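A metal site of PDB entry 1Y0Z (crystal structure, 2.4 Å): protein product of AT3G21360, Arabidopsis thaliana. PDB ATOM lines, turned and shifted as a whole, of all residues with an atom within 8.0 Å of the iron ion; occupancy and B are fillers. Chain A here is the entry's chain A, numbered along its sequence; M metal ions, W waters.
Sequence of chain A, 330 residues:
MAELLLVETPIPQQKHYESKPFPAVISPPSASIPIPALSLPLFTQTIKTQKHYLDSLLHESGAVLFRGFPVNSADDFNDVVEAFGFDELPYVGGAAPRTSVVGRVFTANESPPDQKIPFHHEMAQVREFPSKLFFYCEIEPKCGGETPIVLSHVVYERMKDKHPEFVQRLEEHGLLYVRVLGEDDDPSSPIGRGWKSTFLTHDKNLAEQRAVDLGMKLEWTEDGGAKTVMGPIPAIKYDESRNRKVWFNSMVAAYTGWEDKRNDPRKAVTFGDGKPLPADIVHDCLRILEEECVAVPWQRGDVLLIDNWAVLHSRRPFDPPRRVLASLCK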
ATOM      1  N   ALA A 108     -16.669   9.426  -6.792  1.00  0.00           N
ATOM      2  CA  ALA A 108     -15.350   9.673  -6.262  1.00  0.00           C
ATOM      3  C   ALA A 108     -14.968  11.045  -6.760  1.00  0.00           C
ATOM      4  O   ALA A 108     -15.317  11.439  -7.884  1.00  0.00           O
ATOM      5  CB  ALA A 108     -14.366   8.631  -6.775  1.00  0.00           C
ATOM      6  N   GLU A 110     -12.464  13.379  -8.205  1.00  0.00           N
ATOM      7  CA  GLU A 110     -11.287  13.378  -9.031  1.00  0.00           C
ATOM      8  C   GLU A 110     -10.620  14.731  -8.966  1.00  0.00           C
ATOM      9  O   GLU A 110     -11.036  15.617  -8.224  1.00  0.00           O
ATOM     10  CB  GLU A 110     -11.685  13.100 -10.478  1.00  0.00           C
ATOM     11  CG  GLU A 110     -12.741  12.037 -10.618  1.00  0.00           C
ATOM     12  CD  GLU A 110     -13.275  11.985 -12.025  1.00  0.00           C
ATOM     13  OE1 GLU A 110     -13.784  12.975 -12.550  1.00  0.00           O
ATOM     14  OE2 GLU A 110     -13.169  10.814 -12.646  1.00  0.00           O
ATOM     15  N   ILE A 117      -6.709  13.408 -16.625  1.00  0.00           N
ATOM     16  CA  ILE A 117      -6.383  12.260 -15.789  1.00  0.00           C
ATOM     17  C   ILE A 117      -5.711  11.255 -16.710  1.00  0.00           C
ATOM     18  O   ILE A 117      -6.263  10.879 -17.729  1.00  0.00           O
ATOM     19  CB  ILE A 117      -7.656  11.642 -15.163  1.00  0.00           C
ATOM     20  CG1 ILE A 117      -8.286  12.656 -14.204  1.00  0.00           C
ATOM     21  CG2 ILE A 117      -7.301  10.341 -14.432  1.00  0.00           C
ATOM     22  CD1 ILE A 117      -9.546  12.167 -13.518  1.00  0.00           C
ATOM     23  N   PRO A 118      -4.494  10.807 -16.345  1.00  0.00           N
ATOM     24  CA  PRO A 118      -3.762   9.852 -17.172  1.00  0.00           C
ATOM     25  C   PRO A 118      -4.414   8.474 -17.295  1.00  0.00           C
ATOM     26  O   PRO A 118      -5.325   8.131 -16.548  1.00  0.00           O
ATOM     27  CB  PRO A 118      -2.388   9.764 -16.482  1.00  0.00           C
ATOM     28  CG  PRO A 118      -2.324  10.990 -15.626  1.00  0.00           C
ATOM     29  CD  PRO A 118      -3.741  11.158 -15.142  1.00  0.00           C
ATOM     30  N   PHE A 119      -3.919   7.703 -18.242  1.00  0.00           N
ATOM     31  CA  PHE A 119      -4.395   6.352 -18.473  1.00  0.00           C
ATOM     32  C   PHE A 119      -3.940   5.465 -17.343  1.00  0.00           C
ATOM     33  O   PHE A 119      -2.835   5.612 -16.837  1.00  0.00           O
ATOM     34  CB  PHE A 119      -3.822   5.809 -19.768  1.00  0.00           C
ATOM     35  CG  PHE A 119      -4.580   6.229 -20.971  1.00  0.00           C
ATOM     36  CD1 PHE A 119      -5.830   5.679 -21.247  1.00  0.00           C
ATOM     37  CD2 PHE A 119      -4.062   7.199 -21.817  1.00  0.00           C
ATOM     38  CE1 PHE A 119      -6.546   6.087 -22.354  1.00  0.00           C
ATOM     39  CE2 PHE A 119      -4.789   7.617 -22.925  1.00  0.00           C
ATOM     40  CZ  PHE A 119      -6.024   7.063 -23.192  1.00  0.00           C
ATOM     41  N   HIS A 120      -4.800   4.543 -16.952  1.00  0.00           N
ATOM     42  CA  HIS A 120      -4.482   3.603 -15.884  1.00  0.00           C
ATOM     43  C   HIS A 120      -5.513   2.497 -15.809  1.00  0.00           C
ATOM     44  O   HIS A 120      -6.612   2.600 -16.361  1.00  0.00           O
ATOM     45  CB  HIS A 120      -4.434   4.325 -14.528  1.00  0.00           C
ATOM     46  CG  HIS A 120      -5.752   4.886 -14.102  1.00  0.00           C
ATOM     47  ND1 HIS A 120      -6.344   5.969 -14.721  1.00  0.00           N
ATOM     48  CD2 HIS A 120      -6.594   4.523 -13.100  1.00  0.00           C
ATOM     49  CE1 HIS A 120      -7.478   6.254 -14.115  1.00  0.00           C
ATOM     50  NE2 HIS A 120      -7.651   5.387 -13.129  1.00  0.00           N
ATOM     51  N   HIS A 121      -5.122   1.426 -15.125  1.00  0.00           N
ATOM     52  CA  HIS A 121      -5.998   0.297 -14.870  1.00  0.00           C
ATOM     53  C   HIS A 121      -6.500   0.670 -13.483  1.00  0.00           C
ATOM     54  O   HIS A 121      -5.776   1.277 -12.701  1.00  0.00           O
ATOM     55  CB  HIS A 121      -5.189  -1.008 -14.799  1.00  0.00           C
ATOM     56  CG  HIS A 121      -4.908  -1.611 -16.131  1.00  0.00           C
ATOM     57  ND1 HIS A 121      -5.822  -2.387 -16.812  1.00  0.00           N
ATOM     58  CD2 HIS A 121      -3.819  -1.546 -16.929  1.00  0.00           C
ATOM     59  CE1 HIS A 121      -5.305  -2.769 -17.964  1.00  0.00           C
ATOM     60  NE2 HIS A 121      -4.087  -2.272 -18.060  1.00  0.00           N
ATOM     61  N   GLU A 122      -7.747   0.331 -13.187  1.00  0.00           N
ATOM     62  CA  GLU A 122      -8.328   0.666 -11.892  1.00  0.00           C
ATOM     63  C   GLU A 122      -7.601  -0.060 -10.752  1.00  0.00           C
ATOM     64  O   GLU A 122      -7.435  -1.281 -10.783  1.00  0.00           O
ATOM     65  CB  GLU A 122      -9.812   0.306 -11.890  1.00  0.00           C
ATOM     66  CG  GLU A 122     -10.615   0.986 -10.808  1.00  0.00           C
ATOM     67  CD  GLU A 122     -10.487   2.490 -10.859  1.00  0.00           C
ATOM     68  OE1 GLU A 122     -10.356   3.039 -11.976  1.00  0.00           O
ATOM     69  OE2 GLU A 122     -10.541   3.129  -9.797  1.00  0.00           O
ATOM     70  N   MET A 123      -7.172   0.704  -9.743  1.00  0.00           N
ATOM     71  CA  MET A 123      -6.472   0.162  -8.578  1.00  0.00           C
ATOM     72  C   MET A 123      -5.350  -0.796  -8.985  1.00  0.00           C
ATOM     73  O   MET A 123      -5.186  -1.867  -8.409  1.00  0.00           O
ATOM     74  CB  MET A 123      -7.477  -0.549  -7.670  1.00  0.00           C
ATOM     75  CG  MET A 123      -8.384   0.406  -6.910  1.00  0.00           C
ATOM     76  SD  MET A 123      -9.924  -0.333  -6.343  1.00  0.00           S
ATOM     77  CE  MET A 123      -9.361  -1.319  -4.990  1.00  0.00           C
ATOM     78  N   LEU A 133     -15.405  -2.854 -14.103  1.00  0.00           N
ATOM     79  CA  LEU A 133     -15.934  -1.618 -13.556  1.00  0.00           C
ATOM     80  C   LEU A 133     -17.012  -1.069 -14.482  1.00  0.00           C
ATOM     81  O   LEU A 133     -17.068  -1.396 -15.670  1.00  0.00           O
ATOM     82  CB  LEU A 133     -14.840  -0.573 -13.327  1.00  0.00           C
ATOM     83  CG  LEU A 133     -13.919  -0.090 -14.440  1.00  0.00           C
ATOM     84  CD1 LEU A 133     -13.396   1.289 -14.090  1.00  0.00           C
ATOM     85  CD2 LEU A 133     -12.784  -1.070 -14.615  1.00  0.00           C
ATOM     86  N   PHE A 135     -19.181   2.602 -15.584  1.00  0.00           N
ATOM     87  CA  PHE A 135     -19.214   4.050 -15.555  1.00  0.00           C
ATOM     88  C   PHE A 135     -20.582   4.466 -16.073  1.00  0.00           C
ATOM     89  O   PHE A 135     -21.045   3.956 -17.095  1.00  0.00           O
ATOM     90  CB  PHE A 135     -18.104   4.662 -16.418  1.00  0.00           C
ATOM     91  CG  PHE A 135     -16.765   4.658 -15.759  1.00  0.00           C
ATOM     92  CD1 PHE A 135     -16.609   5.210 -14.498  1.00  0.00           C
ATOM     93  CD2 PHE A 135     -15.653   4.112 -16.400  1.00  0.00           C
ATOM     94  CE1 PHE A 135     -15.371   5.237 -13.877  1.00  0.00           C
ATOM     95  CE2 PHE A 135     -14.399   4.123 -15.788  1.00  0.00           C
ATOM     96  CZ  PHE A 135     -14.259   4.691 -14.517  1.00  0.00           C
ATOM     97  N   THR A 147     -14.393   9.860 -21.418  1.00  0.00           N
ATOM     98  CA  THR A 147     -13.639   8.855 -20.688  1.00  0.00           C
ATOM     99  C   THR A 147     -12.957   7.947 -21.718  1.00  0.00           C
ATOM    100  O   THR A 147     -13.439   6.860 -22.026  1.00  0.00           O
ATOM    101  CB  THR A 147     -14.565   8.061 -19.775  1.00  0.00           C
ATOM    102  OG1 THR A 147     -15.019   8.923 -18.741  1.00  0.00           O
ATOM    103  CG2 THR A 147     -13.858   6.861 -19.157  1.00  0.00           C
ATOM    104  N   ASN A 308     -11.422  -4.637 -16.530  1.00  0.00           N
ATOM    105  CA  ASN A 308     -10.181  -4.051 -16.041  1.00  0.00           C
ATOM    106  C   ASN A 308      -8.897  -4.789 -16.434  1.00  0.00           C
ATOM    107  O   ASN A 308      -7.798  -4.267 -16.287  1.00  0.00           O
ATOM    108  CB  ASN A 308     -10.244  -3.875 -14.528  1.00  0.00           C
ATOM    109  CG  ASN A 308      -9.336  -2.778 -14.039  1.00  0.00           C
ATOM    110  OD1 ASN A 308      -9.248  -1.724 -14.663  1.00  0.00           O
ATOM    111  ND2 ASN A 308      -8.669  -3.005 -12.906  1.00  0.00           N
ATOM    112  N   LEU A 312      -7.511   0.303 -20.121  1.00  0.00           N
ATOM    113  CA  LEU A 312      -7.027   1.369 -19.240  1.00  0.00           C
ATOM    114  C   LEU A 312      -7.936   2.555 -19.565  1.00  0.00           C
ATOM    115  O   LEU A 312      -8.286   2.764 -20.725  1.00  0.00           O
ATOM    116  CB  LEU A 312      -5.567   1.738 -19.542  1.00  0.00           C
ATOM    117  CG  LEU A 312      -4.504   0.645 -19.420  1.00  0.00           C
ATOM    118  CD1 LEU A 312      -4.232   0.026 -20.790  1.00  0.00           C
ATOM    119  CD2 LEU A 312      -3.220   1.249 -18.844  1.00  0.00           C
ATOM    120  N   HIS A 313      -8.329   3.320 -18.560  1.00  0.00           N
ATOM    121  CA  HIS A 313      -9.175   4.458 -18.827  1.00  0.00           C
ATOM    122  C   HIS A 313      -8.560   5.760 -18.345  1.00  0.00           C
ATOM    123  O   HIS A 313      -7.558   5.766 -17.627  1.00  0.00           O
ATOM    124  CB  HIS A 313     -10.558   4.268 -18.195  1.00  0.00           C
ATOM    125  CG  HIS A 313     -10.529   4.174 -16.704  1.00  0.00           C
ATOM    126  ND1 HIS A 313     -10.283   2.996 -16.035  1.00  0.00           N
ATOM    127  CD2 HIS A 313     -10.673   5.127 -15.751  1.00  0.00           C
ATOM    128  CE1 HIS A 313     -10.272   3.218 -14.739  1.00  0.00           C
ATOM    129  NE2 HIS A 313     -10.507   4.506 -14.540  1.00  0.00           N
ATOM    130  N   SER A 314      -9.178   6.873 -18.737  1.00  0.00           N
ATOM    131  CA  SER A 314      -8.719   8.197 -18.363  1.00  0.00           C
ATOM    132  C   SER A 314      -9.881   9.181 -18.371  1.00  0.00           C
ATOM    133  O   SER A 314     -11.045   8.796 -18.463  1.00  0.00           O
ATOM    134  CB  SER A 314      -7.669   8.670 -19.361  1.00  0.00           C
ATOM    135  OG  SER A 314      -8.179   8.596 -20.682  1.00  0.00           O
ATOM    136  N   ARG A 315      -9.541  10.458 -18.269  1.00  0.00           N
ATOM    137  CA  ARG A 315     -10.548  11.493 -18.294  1.00  0.00           C
ATOM    138  C   ARG A 315      -9.963  12.759 -18.921  1.00  0.00           C
ATOM    139  O   ARG A 315      -8.844  13.173 -18.618  1.00  0.00           O
ATOM    140  CB  ARG A 315     -11.076  11.768 -16.885  1.00  0.00           C
ATOM    141  CG  ARG A 315     -12.300  12.659 -16.853  1.00  0.00           C
ATOM    142  CD  ARG A 315     -11.925  14.072 -16.474  1.00  0.00           C
ATOM    143  NE  ARG A 315     -11.847  14.212 -15.027  1.00  0.00           N
ATOM    144  CZ  ARG A 315     -11.265  15.228 -14.401  1.00  0.00           C
ATOM    145  NH1 ARG A 315     -10.675  16.187 -15.084  1.00  0.00           N
ATOM    146  NH2 ARG A 315     -11.251  15.258 -13.082  1.00  0.00           N
ATOM    147  N   ALA A 326     -19.842   5.466 -10.638  1.00  0.00           N
ATOM    148  CA  ALA A 326     -19.122   4.241 -10.913  1.00  0.00           C
ATOM    149  C   ALA A 326     -19.490   3.074 -10.013  1.00  0.00           C
ATOM    150  O   ALA A 326     -20.156   3.232  -8.990  1.00  0.00           O
ATOM    151  CB  ALA A 326     -17.609   4.499 -10.838  1.00  0.00           C
ATOM    152  N   LEU A 328     -17.583  -0.883  -8.928  1.00  0.00           N
ATOM    153  CA  LEU A 328     -16.484  -1.828  -9.096  1.00  0.00           C
ATOM    154  C   LEU A 328     -16.871  -3.270  -8.806  1.00  0.00           C
ATOM    155  O   LEU A 328     -17.618  -3.551  -7.867  1.00  0.00           O
ATOM    156  CB  LEU A 328     -15.318  -1.421  -8.174  1.00  0.00           C
ATOM    157  CG  LEU A 328     -14.780   0.002  -8.369  1.00  0.00           C
ATOM    158  CD1 LEU A 328     -13.780   0.364  -7.260  1.00  0.00           C
ATOM    159  CD2 LEU A 328     -14.121   0.095  -9.736  1.00  0.00           C
HETATM  160 FE    FE M   1      -9.948   5.536 -12.574  1.00  0.00          FE
HETATM  161  O   HOH W   1     -12.107   5.635 -11.697  1.00  0.00           O
HETATM  162  O   HOH W   2      -9.543   8.400 -11.661  1.00  0.00           O
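O of Pro 118 is in hydrogen-bond range of ND1 of His 120, 3.0 Å away.
The backbone NH (N) of Glu 122 sits at hydrogen-bond distance from the side-chain amide oxygen (OD1) of Asn 308, 2.9 Å away.
The iron ion is bound by a ring nitrogen (NE2) of His 313 (2.3 Å), water W1 (2.3 Å), a ring nitrogen (NE2) of His 120 (2.4 Å) and the side-chain carboxylate of Glu 122 (2.6 Å).
The iron ion has four donor atoms within binding distance.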
